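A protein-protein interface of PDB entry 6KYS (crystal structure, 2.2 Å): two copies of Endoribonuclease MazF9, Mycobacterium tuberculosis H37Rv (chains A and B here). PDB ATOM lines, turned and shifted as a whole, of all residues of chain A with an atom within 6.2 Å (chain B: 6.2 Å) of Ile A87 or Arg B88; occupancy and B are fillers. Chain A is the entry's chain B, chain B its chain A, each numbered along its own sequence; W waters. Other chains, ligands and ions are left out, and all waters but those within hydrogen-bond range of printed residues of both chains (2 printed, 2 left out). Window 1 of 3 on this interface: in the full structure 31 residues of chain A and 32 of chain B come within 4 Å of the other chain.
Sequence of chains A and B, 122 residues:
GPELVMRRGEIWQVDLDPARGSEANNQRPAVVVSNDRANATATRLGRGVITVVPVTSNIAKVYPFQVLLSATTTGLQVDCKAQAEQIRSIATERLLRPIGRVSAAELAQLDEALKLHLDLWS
Of the 19 printed residues of chain B, 10 touch a printed residue of chain A.
Printed residues of chain B that touch a printed residue of chain A: Pro B18, Glu B23, Thr B51, Gln B86, Ile B87, Arg B88, Ser B89, Ile B90, Arg B94 and Leu B118.
Printed residues of chain A that touch a printed residue of chain B: Pro A18, Glu A23, Val A33, Thr A51, Glu A85, Gln A86, Ile A87, Arg A88, Ser A89, Arg A94, His A117 and Leu A118.
Hydrophobic or aromatic side chains of chain A within 4 Å of the printed part of chain B: Pro A18, Val A33, Ile A87, His A117 and Leu A118.
Among the printed residues, 18 pairs touch across the chains.
Among the printed residues, Asp or Glu carboxylates within 4 Å of a Lys or Arg side-chain nitrogen of the other chain: Glu A23 with Arg B94 (2.7 Å) and Arg A94 with Glu B23 (2.7 Å).
Water W1 lies within hydrogen-bond range of the backbone carbonyl oxygen (O) of Glu A85 (2.7 Å), the side-chain hydroxyl (OG1) of Thr B51 (2.9 Å) and a ring nitrogen (NE2) of His A117 (3.4 Å).
Water W2 lies within hydrogen-bond range of OE1 of Glu B23 (2.8 Å), NH2 of Arg A88 (3.0 Å) and NH1 of Arg B88 (3.1 Å).
Glu A23 touches Arg B94, and with the chains exchanged Arg A94 touches Glu B23.
Ile A87 touches Arg B88, and with the chains exchanged Arg A88 touches Ile B87.
Ile A87 touches Ser B89, and with the chains exchanged Ser A89 touches Ile B87.
Leu B118 touches its own counterpart, Leu A118.
13 positions are printed for both chains.
Of the 18 pairs that touch across the chains among the printed residues, 13 have their exchanged pair printed and touching as well.
Among the printed residues, merely in contact across the chains: Pro A18 with Pro B18 (3.4 Å), Glu A23 with Ile B90 (3.4 Å), Gln A86 with Ser B89 (3.6 Å), Ser A89 with Gln B86 (3.6 Å), Arg A88 with Arg B88 (3.7 Å), Thr A51 with Leu B118 (3.7 Å), Leu A118 with Leu B118 (3.7 Å), Leu A118 with Thr B51 (3.8 Å), Arg A88 with Ile B87 (3.8 Å), Ile A87 with Arg B88 (3.8 Å) and Leu A118 with Ile B87 (3.8 Å).
Printed residues of chain B within 4 Å of Ile A87: Arg B88 and Ser B89.
Of the printed residues of chain B, Arg A94 touches Glu B23 (2.7 Å).
Val B53 touches none of the printed residues of chain A.
Of the printed residues of chain A, Gln B86 touches Ser A89 (3.6 Å).
Of the printed residues of chain A, Ile B87 touches Arg A88, Ser A89 and Leu A118.
Printed residues of chain A within 4 Å of Ile B90: Glu A23.
The guanidinium group of Arg B94 is in hydrogen-bond range of the backbone carbonyl oxygen of Asp B15, 3.0 Å away.
O of Ile B50 lies within hydrogen-bond range of N of Ile B90, 2.8 Å away.
The side-chain hydroxyl (OG) of Ser B89 sits at hydrogen-bond distance from the side-chain hydroxyl (OG1) of Thr B51.
The backbone NH (N) of Val B52 is in hydrogen-bond range of the backbone carbonyl oxygen (O) of Arg B88.
NE of Arg A94 is in salt-bridge range of OE2 of Glu B23 (2.7 Å).
The side-chain hydroxyl of Thr B51 sits at hydrogen-bond distance from a ring nitrogen (NE2) of His A117.
The backbone carbonyl oxygen (O) of Ile B87 lies within hydrogen-bond range of the backbone NH (N) of Ser A89, 2.9 Å away.
OG of Ser B89 is in hydrogen-bond range of O of Glu A85 (3.0 Å).
The backbone carbonyl oxygen of Ile A87 is in hydrogen-bond range of the side-chain hydroxyl of Ser B89 (2.9 Å).
The side-chain carboxylate (OE2) of Glu A23 lies within salt-bridge range of the guanidinium group (NE) of Arg B94, at 2.7 Å.
O of Leu B118 sits close to O of Val A33 (3.4 Å).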
ATOM      1  N   PRO A  18     -15.248 -21.849  -4.740  1.00  0.00           N
ATOM      2  CA  PRO A  18     -16.542 -21.479  -4.154  1.00  0.00           C
ATOM      3  C   PRO A  18     -16.409 -21.032  -2.705  1.00  0.00           C
ATOM      4  O   PRO A  18     -15.445 -21.407  -2.044  1.00  0.00           O
ATOM      5  CB  PRO A  18     -17.352 -22.768  -4.264  1.00  0.00           C
ATOM      6  CG  PRO A  18     -16.334 -23.834  -4.153  1.00  0.00           C
ATOM      7  CD  PRO A  18     -15.066 -23.311  -4.782  1.00  0.00           C
ATOM      8  N   ALA A  19     -17.364 -20.233  -2.229  1.00  0.00           N
ATOM      9  CA  ALA A  19     -17.313 -19.650  -0.897  1.00  0.00           C
ATOM     10  C   ALA A  19     -18.644 -19.863  -0.191  1.00  0.00           C
ATOM     11  O   ALA A  19     -19.677 -20.091  -0.828  1.00  0.00           O
ATOM     12  CB  ALA A  19     -16.984 -18.152  -0.956  1.00  0.00           C
ATOM     13  N   GLU A  23     -17.869 -15.235   3.469  1.00  0.00           N
ATOM     14  CA  GLU A  23     -16.554 -15.322   2.857  1.00  0.00           C
ATOM     15  C   GLU A  23     -16.511 -14.496   1.576  1.00  0.00           C
ATOM     16  O   GLU A  23     -17.441 -14.534   0.764  1.00  0.00           O
ATOM     17  CB  GLU A  23     -16.201 -16.790   2.582  1.00  0.00           C
ATOM     18  CG  GLU A  23     -15.941 -17.594   3.861  1.00  0.00           C
ATOM     19  CD  GLU A  23     -15.999 -19.110   3.674  1.00  0.00           C
ATOM     20  OE1 GLU A  23     -16.140 -19.579   2.524  1.00  0.00           O
ATOM     21  OE2 GLU A  23     -15.919 -19.830   4.699  1.00  0.00           O
ATOM     22  N   VAL A  33       0.340 -10.918   1.606  1.00  0.00           N
ATOM     23  CA  VAL A  33       0.844 -10.556   2.928  1.00  0.00           C
ATOM     24  C   VAL A  33       1.743 -11.642   3.505  1.00  0.00           C
ATOM     25  O   VAL A  33       2.308 -11.469   4.590  1.00  0.00           O
ATOM     26  CB  VAL A  33      -0.307 -10.251   3.905  1.00  0.00           C
ATOM     27  CG1 VAL A  33      -1.094  -9.035   3.443  1.00  0.00           C
ATOM     28  CG2 VAL A  33      -1.217 -11.470   4.060  1.00  0.00           C
ATOM     29  N   THR A  51      -0.630 -16.299   1.218  1.00  0.00           N
ATOM     30  CA  THR A  51      -1.599 -15.677   2.110  1.00  0.00           C
ATOM     31  C   THR A  51      -1.937 -14.288   1.590  1.00  0.00           C
ATOM     32  O   THR A  51      -1.035 -13.482   1.322  1.00  0.00           O
ATOM     33  CB  THR A  51      -1.072 -15.603   3.542  1.00  0.00           C
ATOM     34  OG1 THR A  51      -0.669 -16.908   3.966  1.00  0.00           O
ATOM     35  CG2 THR A  51      -2.170 -15.109   4.474  1.00  0.00           C
ATOM     36  N   VAL A  52      -3.237 -14.017   1.424  1.00  0.00           N
ATOM     37  CA  VAL A  52      -3.699 -12.759   0.852  1.00  0.00           C
ATOM     38  C   VAL A  52      -4.796 -12.172   1.732  1.00  0.00           C
ATOM     39  O   VAL A  52      -5.380 -12.846   2.590  1.00  0.00           O
ATOM     40  CB  VAL A  52      -4.199 -12.910  -0.614  1.00  0.00           C
ATOM     41  CG1 VAL A  52      -3.120 -13.531  -1.501  1.00  0.00           C
ATOM     42  CG2 VAL A  52      -5.475 -13.729  -0.686  1.00  0.00           C
ATOM     43  N   VAL A  53      -5.054 -10.883   1.512  1.00  0.00           N
ATOM     44  CA  VAL A  53      -6.119 -10.120   2.138  1.00  0.00           C
ATOM     45  C   VAL A  53      -7.071  -9.667   1.024  1.00  0.00           C
ATOM     46  O   VAL A  53      -6.705  -8.804   0.214  1.00  0.00           O
ATOM     47  CB  VAL A  53      -5.578  -8.920   2.928  1.00  0.00           C
ATOM     48  CG1 VAL A  53      -6.703  -7.968   3.296  1.00  0.00           C
ATOM     49  CG2 VAL A  53      -4.865  -9.393   4.181  1.00  0.00           C
ATOM     50  N   PRO A  54      -8.266 -10.243   0.926  1.00  0.00           N
ATOM     51  CA  PRO A  54      -9.197  -9.841  -0.134  1.00  0.00           C
ATOM     52  C   PRO A  54      -9.648  -8.394   0.013  1.00  0.00           C
ATOM     53  O   PRO A  54      -9.566  -7.777   1.079  1.00  0.00           O
ATOM     54  CB  PRO A  54     -10.372 -10.813   0.034  1.00  0.00           C
ATOM     55  CG  PRO A  54      -9.772 -12.008   0.710  1.00  0.00           C
ATOM     56  CD  PRO A  54      -8.715 -11.457   1.628  1.00  0.00           C
ATOM     57  N   GLN A  83      -9.567  -6.117   3.603  1.00  0.00           N
ATOM     58  CA  GLN A  83     -10.297  -6.671   4.742  1.00  0.00           C
ATOM     59  C   GLN A  83      -9.417  -7.701   5.436  1.00  0.00           C
ATOM     60  O   GLN A  83      -9.384  -8.869   5.036  1.00  0.00           O
ATOM     61  CB  GLN A  83     -11.604  -7.303   4.284  1.00  0.00           C
ATOM     62  CG  GLN A  83     -12.587  -6.347   3.649  1.00  0.00           C
ATOM     63  CD  GLN A  83     -13.808  -7.073   3.137  1.00  0.00           C
ATOM     64  OE1 GLN A  83     -14.802  -7.211   3.845  1.00  0.00           O
ATOM     65  NE2 GLN A  83     -13.732  -7.563   1.911  1.00  0.00           N
ATOM     66  N   ALA A  84      -8.714  -7.269   6.487  1.00  0.00           N
ATOM     67  CA  ALA A  84      -7.850  -8.187   7.223  1.00  0.00           C
ATOM     68  C   ALA A  84      -8.636  -9.345   7.820  1.00  0.00           C
ATOM     69  O   ALA A  84      -8.092 -10.444   7.981  1.00  0.00           O
ATOM     70  CB  ALA A  84      -7.096  -7.444   8.325  1.00  0.00           C
ATOM     71  N   GLU A  85      -9.912  -9.124   8.148  1.00  0.00           N
ATOM     72  CA  GLU A  85     -10.742 -10.180   8.711  1.00  0.00           C
ATOM     73  C   GLU A  85     -11.103 -11.249   7.686  1.00  0.00           C
ATOM     74  O   GLU A  85     -11.672 -12.278   8.065  1.00  0.00           O
ATOM     75  CB  GLU A  85     -12.011  -9.577   9.325  1.00  0.00           C
ATOM     76  CG  GLU A  85     -13.132  -9.242   8.332  1.00  0.00           C
ATOM     77  CD  GLU A  85     -12.910  -7.948   7.560  1.00  0.00           C
ATOM     78  OE1 GLU A  85     -11.809  -7.367   7.649  1.00  0.00           O
ATOM     79  OE2 GLU A  85     -13.855  -7.507   6.867  1.00  0.00           O
ATOM     80  N   GLN A  86     -10.784 -11.031   6.410  1.00  0.00           N
ATOM     81  CA  GLN A  86     -10.976 -12.016   5.354  1.00  0.00           C
ATOM     82  C   GLN A  86      -9.670 -12.687   4.937  1.00  0.00           C
ATOM     83  O   GLN A  86      -9.640 -13.358   3.901  1.00  0.00           O
ATOM     84  CB  GLN A  86     -11.632 -11.360   4.137  1.00  0.00           C
ATOM     85  CG  GLN A  86     -13.044 -10.831   4.379  1.00  0.00           C
ATOM     86  CD  GLN A  86     -14.089 -11.927   4.297  1.00  0.00           C
ATOM     87  OE1 GLN A  86     -13.788 -13.051   3.888  1.00  0.00           O
ATOM     88  NE2 GLN A  86     -15.325 -11.609   4.683  1.00  0.00           N
ATOM     89  N   ILE A  87      -8.595 -12.520   5.718  1.00  0.00           N
ATOM     90  CA  ILE A  87      -7.299 -13.096   5.369  1.00  0.00           C
ATOM     91  C   ILE A  87      -7.447 -14.584   5.054  1.00  0.00           C
ATOM     92  O   ILE A  87      -8.187 -15.309   5.727  1.00  0.00           O
ATOM     93  CB  ILE A  87      -6.290 -12.851   6.509  1.00  0.00           C
ATOM     94  CG1 ILE A  87      -4.909 -13.407   6.145  1.00  0.00           C
ATOM     95  CG2 ILE A  87      -6.794 -13.451   7.828  1.00  0.00           C
ATOM     96  CD1 ILE A  87      -3.818 -13.029   7.121  1.00  0.00           C
ATOM     97  N   ARG A  88      -6.758 -15.037   4.004  1.00  0.00           N
ATOM     98  CA  ARG A  88      -6.918 -16.412   3.541  1.00  0.00           C
ATOM     99  C   ARG A  88      -5.676 -16.883   2.794  1.00  0.00           C
ATOM    100  O   ARG A  88      -5.142 -16.168   1.940  1.00  0.00           O
ATOM    101  CB  ARG A  88      -8.152 -16.552   2.636  1.00  0.00           C
ATOM    102  CG  ARG A  88      -8.322 -17.943   2.017  1.00  0.00           C
ATOM    103  CD  ARG A  88      -9.575 -18.030   1.149  1.00  0.00           C
ATOM    104  NE  ARG A  88      -9.782 -19.378   0.623  1.00  0.00           N
ATOM    105  CZ  ARG A  88     -10.685 -19.694  -0.305  1.00  0.00           C
ATOM    106  NH1 ARG A  88     -11.478 -18.759  -0.815  1.00  0.00           N
ATOM    107  NH2 ARG A  88     -10.798 -20.947  -0.721  1.00  0.00           N
ATOM    108  N   SER A  89      -5.231 -18.098   3.118  1.00  0.00           N
ATOM    109  CA  SER A  89      -4.160 -18.766   2.390  1.00  0.00           C
ATOM    110  C   SER A  89      -4.750 -19.513   1.197  1.00  0.00           C
ATOM    111  O   SER A  89      -5.644 -20.349   1.365  1.00  0.00           O
ATOM    112  CB  SER A  89      -3.413 -19.734   3.309  1.00  0.00           C
ATOM    113  OG  SER A  89      -2.767 -19.033   4.358  1.00  0.00           O
ATOM    114  N   ARG A  94      -4.904 -20.470  -7.878  1.00  0.00           N
ATOM    115  CA  ARG A  94      -5.975 -19.481  -7.852  1.00  0.00           C
ATOM    116  C   ARG A  94      -5.548 -18.101  -8.355  1.00  0.00           C
ATOM    117  O   ARG A  94      -6.401 -17.210  -8.462  1.00  0.00           O
ATOM    118  CB  ARG A  94      -6.518 -19.323  -6.429  1.00  0.00           C
ATOM    119  CG  ARG A  94      -7.307 -20.521  -5.897  1.00  0.00           C
ATOM    120  CD  ARG A  94      -7.829 -20.240  -4.490  1.00  0.00           C
ATOM    121  NE  ARG A  94      -8.487 -21.397  -3.885  1.00  0.00           N
ATOM    122  CZ  ARG A  94      -9.779 -21.688  -4.023  1.00  0.00           C
ATOM    123  NH1 ARG A  94     -10.570 -20.910  -4.752  1.00  0.00           N
ATOM    124  NH2 ARG A  94     -10.283 -22.758  -3.428  1.00  0.00           N
ATOM    125  N   LEU A 114      -3.758  -6.432  10.602  1.00  0.00           N
ATOM    126  CA  LEU A 114      -3.589  -7.868  10.810  1.00  0.00           C
ATOM    127  C   LEU A 114      -3.229  -8.185  12.257  1.00  0.00           C
ATOM    128  O   LEU A 114      -3.775  -9.126  12.850  1.00  0.00           O
ATOM    129  CB  LEU A 114      -2.512  -8.413   9.874  1.00  0.00           C
ATOM    130  CG  LEU A 114      -2.907  -8.546   8.409  1.00  0.00           C
ATOM    131  CD1 LEU A 114      -1.689  -8.945   7.585  1.00  0.00           C
ATOM    132  CD2 LEU A 114      -4.032  -9.559   8.266  1.00  0.00           C
ATOM    133  N   HIS A 117      -6.339  -7.839  14.234  1.00  0.00           N
ATOM    134  CA  HIS A 117      -7.364  -8.845  13.990  1.00  0.00           C
ATOM    135  C   HIS A 117      -6.984 -10.185  14.603  1.00  0.00           C
ATOM    136  O   HIS A 117      -7.843 -10.883  15.157  1.00  0.00           O
ATOM    137  CB  HIS A 117      -7.609  -8.993  12.488  1.00  0.00           C
ATOM    138  CG  HIS A 117      -8.502 -10.141  12.143  1.00  0.00           C
ATOM    139  ND1 HIS A 117      -9.821 -10.201  12.541  1.00  0.00           N
ATOM    140  CD2 HIS A 117      -8.264 -11.284  11.456  1.00  0.00           C
ATOM    141  CE1 HIS A 117     -10.358 -11.330  12.111  1.00  0.00           C
ATOM    142  NE2 HIS A 117      -9.434 -12.004  11.448  1.00  0.00           N
ATOM    143  N   LEU A 118      -5.704 -10.555  14.518  1.00  0.00           N
ATOM    144  CA  LEU A 118      -5.215 -11.830  15.028  1.00  0.00           C
ATOM    145  C   LEU A 118      -4.678 -11.729  16.453  1.00  0.00           C
ATOM    146  O   LEU A 118      -4.096 -12.700  16.954  1.00  0.00           O
ATOM    147  CB  LEU A 118      -4.135 -12.395  14.094  1.00  0.00           C
ATOM    148  CG  LEU A 118      -4.569 -12.668  12.644  1.00  0.00           C
ATOM    149  CD1 LEU A 118      -3.371 -12.985  11.761  1.00  0.00           C
ATOM    150  CD2 LEU A 118      -5.611 -13.779  12.561  1.00  0.00           C
ATOM    151  N   ASP B  15     -15.013 -27.757   8.515  1.00  0.00           N
ATOM    152  CA  ASP B  15     -15.217 -28.276   7.167  1.00  0.00           C
ATOM    153  C   ASP B  15     -14.544 -27.328   6.179  1.00  0.00           C
ATOM    154  O   ASP B  15     -15.018 -26.207   5.965  1.00  0.00           O
ATOM    155  CB  ASP B  15     -16.712 -28.417   6.877  1.00  0.00           C
ATOM    156  CG  ASP B  15     -17.000 -28.904   5.470  1.00  0.00           C
ATOM    157  OD1 ASP B  15     -16.086 -29.463   4.820  1.00  0.00           O
ATOM    158  OD2 ASP B  15     -18.154 -28.729   5.018  1.00  0.00           O
ATOM    159  N   LEU B  16     -13.447 -27.777   5.575  1.00  0.00           N
ATOM    160  CA  LEU B  16     -12.655 -26.941   4.682  1.00  0.00           C
ATOM    161  C   LEU B  16     -12.933 -27.195   3.206  1.00  0.00           C
ATOM    162  O   LEU B  16     -12.310 -26.550   2.358  1.00  0.00           O
ATOM    163  CB  LEU B  16     -11.165 -27.148   4.957  1.00  0.00           C
ATOM    164  CG  LEU B  16     -10.692 -26.775   6.357  1.00  0.00           C
ATOM    165  CD1 LEU B  16      -9.207 -27.061   6.490  1.00  0.00           C
ATOM    166  CD2 LEU B  16     -10.986 -25.312   6.639  1.00  0.00           C
ATOM    167  N   ASP B  17     -13.845 -28.108   2.879  1.00  0.00           N
ATOM    168  CA  ASP B  17     -14.113 -28.471   1.488  1.00  0.00           C
ATOM    169  C   ASP B  17     -15.076 -27.495   0.808  1.00  0.00           C
ATOM    170  O   ASP B  17     -15.956 -26.932   1.456  1.00  0.00           O
ATOM    171  CB  ASP B  17     -14.679 -29.893   1.413  1.00  0.00           C
ATOM    172  CG  ASP B  17     -13.604 -30.956   1.484  1.00  0.00           C
ATOM    173  OD1 ASP B  17     -12.432 -30.648   1.173  1.00  0.00           O
ATOM    174  OD2 ASP B  17     -13.935 -32.102   1.858  1.00  0.00           O
ATOM    175  N   PRO B  18     -14.908 -27.291  -0.508  1.00  0.00           N
ATOM    176  CA  PRO B  18     -13.812 -27.861  -1.305  1.00  0.00           C
ATOM    177  C   PRO B  18     -12.555 -26.998  -1.289  1.00  0.00           C
ATOM    178  O   PRO B  18     -12.634 -25.783  -1.091  1.00  0.00           O
ATOM    179  CB  PRO B  18     -14.408 -27.929  -2.714  1.00  0.00           C
ATOM    180  CG  PRO B  18     -15.364 -26.805  -2.761  1.00  0.00           C
ATOM    181  CD  PRO B  18     -15.906 -26.613  -1.355  1.00  0.00           C
ATOM    182  N   ALA B  19     -11.403 -27.631  -1.490  1.00  0.00           N
ATOM    183  CA  ALA B  19     -10.122 -26.944  -1.537  1.00  0.00           C
ATOM    184  C   ALA B  19      -9.444 -27.206  -2.877  1.00  0.00           C
ATOM    185  O   ALA B  19      -9.809 -28.133  -3.609  1.00  0.00           O
ATOM    186  CB  ALA B  19      -9.212 -27.390  -0.384  1.00  0.00           C
ATOM    187  N   GLU B  23      -3.972 -26.378  -0.569  1.00  0.00           N
ATOM    188  CA  GLU B  23      -4.797 -25.902   0.532  1.00  0.00           C
ATOM    189  C   GLU B  23      -5.242 -27.071   1.407  1.00  0.00           C
ATOM    190  O   GLU B  23      -5.613 -28.135   0.904  1.00  0.00           O
ATOM    191  CB  GLU B  23      -6.018 -25.157  -0.010  1.00  0.00           C
ATOM    192  CG  GLU B  23      -5.687 -23.835  -0.681  1.00  0.00           C
ATOM    193  CD  GLU B  23      -6.833 -23.300  -1.530  1.00  0.00           C
ATOM    194  OE1 GLU B  23      -7.891 -23.965  -1.607  1.00  0.00           O
ATOM    195  OE2 GLU B  23      -6.676 -22.209  -2.118  1.00  0.00           O
ATOM    196  N   ALA B  24      -5.188 -26.873   2.723  1.00  0.00           N
ATOM    197  CA  ALA B  24      -5.737 -27.856   3.652  1.00  0.00           C
ATOM    198  C   ALA B  24      -7.188 -28.165   3.296  1.00  0.00           C
ATOM    199  O   ALA B  24      -7.980 -27.262   3.009  1.00  0.00           O
ATOM    200  CB  ALA B  24      -5.646 -27.341   5.092  1.00  0.00           C
ATOM    201  N   ILE B  50     -14.673 -15.999  11.141  1.00  0.00           N
ATOM    202  CA  ILE B  50     -13.680 -16.146  12.195  1.00  0.00           C
ATOM    203  C   ILE B  50     -12.434 -16.716  11.538  1.00  0.00           C
ATOM    204  O   ILE B  50     -12.521 -17.412  10.525  1.00  0.00           O
ATOM    205  CB  ILE B  50     -14.173 -17.066  13.335  1.00  0.00           C
ATOM    206  CG1 ILE B  50     -14.637 -18.410  12.761  1.00  0.00           C
ATOM    207  CG2 ILE B  50     -15.294 -16.402  14.122  1.00  0.00           C
ATOM    208  CD1 ILE B  50     -14.346 -19.600  13.651  1.00  0.00           C
ATOM    209  N   THR B  51     -11.268 -16.419  12.097  1.00  0.00           N
ATOM    210  CA  THR B  51     -10.021 -16.866  11.489  1.00  0.00           C
ATOM    211  C   THR B  51      -9.460 -18.049  12.271  1.00  0.00           C
ATOM    212  O   THR B  51      -9.412 -18.017  13.506  1.00  0.00           O
ATOM    213  CB  THR B  51      -8.997 -15.731  11.417  1.00  0.00           C
ATOM    214  OG1 THR B  51      -9.569 -14.613  10.726  1.00  0.00           O
ATOM    215  CG2 THR B  51      -7.762 -16.198  10.651  1.00  0.00           C
ATOM    216  N   VAL B  52      -9.049 -19.095  11.548  1.00  0.00           N
ATOM    217  CA  VAL B  52      -8.553 -20.325  12.152  1.00  0.00           C
ATOM    218  C   VAL B  52      -7.277 -20.761  11.443  1.00  0.00           C
ATOM    219  O   VAL B  52      -7.041 -20.440  10.275  1.00  0.00           O
ATOM    220  CB  VAL B  52      -9.594 -21.472  12.112  1.00  0.00           C
ATOM    221  CG1 VAL B  52     -10.902 -21.053  12.776  1.00  0.00           C
ATOM    222  CG2 VAL B  52      -9.834 -21.942  10.672  1.00  0.00           C
ATOM    223  N   VAL B  53      -6.456 -21.508  12.175  1.00  0.00           N
ATOM    224  CA  VAL B  53      -5.239 -22.132  11.667  1.00  0.00           C
ATOM    225  C   VAL B  53      -5.475 -23.639  11.632  1.00  0.00           C
ATOM    226  O   VAL B  53      -5.581 -24.277  12.694  1.00  0.00           O
ATOM    227  CB  VAL B  53      -4.011 -21.779  12.516  1.00  0.00           C
ATOM    228  CG1 VAL B  53      -2.823 -22.660  12.120  1.00  0.00           C
ATOM    229  CG2 VAL B  53      -3.661 -20.308  12.359  1.00  0.00           C
ATOM    230  N   PRO B  54      -5.576 -24.246  10.449  1.00  0.00           N
ATOM    231  CA  PRO B  54      -5.797 -25.692  10.363  1.00  0.00           C
ATOM    232  C   PRO B  54      -4.653 -26.494  10.963  1.00  0.00           C
ATOM    233  O   PRO B  54      -3.519 -26.026  11.103  1.00  0.00           O
ATOM    234  CB  PRO B  54      -5.915 -25.943   8.854  1.00  0.00           C
ATOM    235  CG  PRO B  54      -6.377 -24.635   8.298  1.00  0.00           C
ATOM    236  CD  PRO B  54      -5.684 -23.594   9.134  1.00  0.00           C
ATOM    237  N   GLN B  86      -1.282 -22.064   6.578  1.00  0.00           N
ATOM    238  CA  GLN B  86      -2.600 -22.447   6.085  1.00  0.00           C
ATOM    239  C   GLN B  86      -3.717 -21.607   6.702  1.00  0.00           C
ATOM    240  O   GLN B  86      -4.891 -21.974   6.585  1.00  0.00           O
ATOM    241  CB  GLN B  86      -2.850 -23.934   6.351  1.00  0.00           C
ATOM    242  CG  GLN B  86      -1.911 -24.886   5.604  1.00  0.00           C
ATOM    243  CD  GLN B  86      -2.371 -25.167   4.181  1.00  0.00           C
ATOM    244  OE1 GLN B  86      -3.486 -24.810   3.802  1.00  0.00           O
ATOM    245  NE2 GLN B  86      -1.513 -25.810   3.387  1.00  0.00           N
ATOM    246  N   ILE B  87      -3.375 -20.486   7.351  1.00  0.00           N
ATOM    247  CA  ILE B  87      -4.371 -19.665   8.034  1.00  0.00           C
ATOM    248  C   ILE B  87      -5.501 -19.303   7.075  1.00  0.00           C
ATOM    249  O   ILE B  87      -5.270 -18.972   5.906  1.00  0.00           O
ATOM    250  CB  ILE B  87      -3.710 -18.407   8.633  1.00  0.00           C
ATOM    251  CG1 ILE B  87      -4.731 -17.567   9.407  1.00  0.00           C
ATOM    252  CG2 ILE B  87      -3.051 -17.551   7.551  1.00  0.00           C
ATOM    253  CD1 ILE B  87      -4.125 -16.399  10.156  1.00  0.00           C
ATOM    254  N   ARG B  88      -6.737 -19.382   7.573  1.00  0.00           N
ATOM    255  CA  ARG B  88      -7.911 -19.170   6.732  1.00  0.00           C
ATOM    256  C   ARG B  88      -9.046 -18.559   7.543  1.00  0.00           C
ATOM    257  O   ARG B  88      -9.328 -19.008   8.658  1.00  0.00           O
ATOM    258  CB  ARG B  88      -8.369 -20.491   6.101  1.00  0.00           C
ATOM    259  CG  ARG B  88      -9.653 -20.377   5.299  1.00  0.00           C
ATOM    260  CD  ARG B  88      -9.979 -21.662   4.574  1.00  0.00           C
ATOM    261  NE  ARG B  88     -11.107 -21.479   3.668  1.00  0.00           N
ATOM    262  CZ  ARG B  88     -11.669 -22.457   2.966  1.00  0.00           C
ATOM    263  NH1 ARG B  88     -11.210 -23.703   3.062  1.00  0.00           N
ATOM    264  NH2 ARG B  88     -12.693 -22.190   2.168  1.00  0.00           N
ATOM    265  N   SER B  89      -9.695 -17.542   6.974  1.00  0.00           N
ATOM    266  CA  SER B  89     -10.929 -16.993   7.524  1.00  0.00           C
ATOM    267  C   SER B  89     -12.119 -17.757   6.961  1.00  0.00           C
ATOM    268  O   SER B  89     -12.252 -17.904   5.741  1.00  0.00           O
ATOM    269  CB  SER B  89     -11.065 -15.509   7.191  1.00  0.00           C
ATOM    270  OG  SER B  89     -10.072 -14.751   7.858  1.00  0.00           O
ATOM    271  N   ILE B  90     -12.994 -18.214   7.850  1.00  0.00           N
ATOM    272  CA  ILE B  90     -14.090 -19.106   7.503  1.00  0.00           C
ATOM    273  C   ILE B  90     -15.408 -18.525   7.995  1.00  0.00           C
ATOM    274  O   ILE B  90     -15.466 -17.804   8.999  1.00  0.00           O
ATOM    275  CB  ILE B  90     -13.867 -20.520   8.091  1.00  0.00           C
ATOM    276  CG1 ILE B  90     -13.678 -20.443   9.611  1.00  0.00           C
ATOM    277  CG2 ILE B  90     -12.663 -21.190   7.442  1.00  0.00           C
ATOM    278  CD1 ILE B  90     -13.547 -21.794  10.286  1.00  0.00           C
ATOM    279  N   ARG B  94     -18.989 -23.185   8.934  1.00  0.00           N
ATOM    280  CA  ARG B  94     -18.040 -24.275   8.749  1.00  0.00           C
ATOM    281  C   ARG B  94     -17.618 -24.906  10.067  1.00  0.00           C
ATOM    282  O   ARG B  94     -16.956 -25.951  10.048  1.00  0.00           O
ATOM    283  CB  ARG B  94     -16.796 -23.796   7.995  1.00  0.00           C
ATOM    284  CG  ARG B  94     -17.009 -23.472   6.517  1.00  0.00           C
ATOM    285  CD  ARG B  94     -15.684 -23.067   5.874  1.00  0.00           C
ATOM    286  NE  ARG B  94     -15.846 -22.533   4.524  1.00  0.00           N
ATOM    287  CZ  ARG B  94     -15.788 -23.260   3.412  1.00  0.00           C
ATOM    288  NH1 ARG B  94     -15.568 -24.569   3.475  1.00  0.00           N
ATOM    289  NH2 ARG B  94     -15.950 -22.672   2.232  1.00  0.00           N
ATOM    290  N   LEU B 118       3.719 -14.101   8.509  1.00  0.00           N
ATOM    291  CA  LEU B 118       3.123 -12.907   7.924  1.00  0.00           C
ATOM    292  C   LEU B 118       4.038 -11.694   8.003  1.00  0.00           C
ATOM    293  O   LEU B 118       3.625 -10.592   7.621  1.00  0.00           O
ATOM    294  CB  LEU B 118       1.783 -12.601   8.598  1.00  0.00           C
ATOM    295  CG  LEU B 118       0.671 -13.651   8.446  1.00  0.00           C
ATOM    296  CD1 LEU B 118      -0.470 -13.396   9.427  1.00  0.00           C
ATOM    297  CD2 LEU B 118       0.143 -13.685   7.011  1.00  0.00           C
HETATM  298  O   HOH W   1     -12.243 -13.574  10.374  1.00  0.00           O
HETATM  299  O   HOH W   2      -9.454 -23.244   0.566  1.00  0.00           O
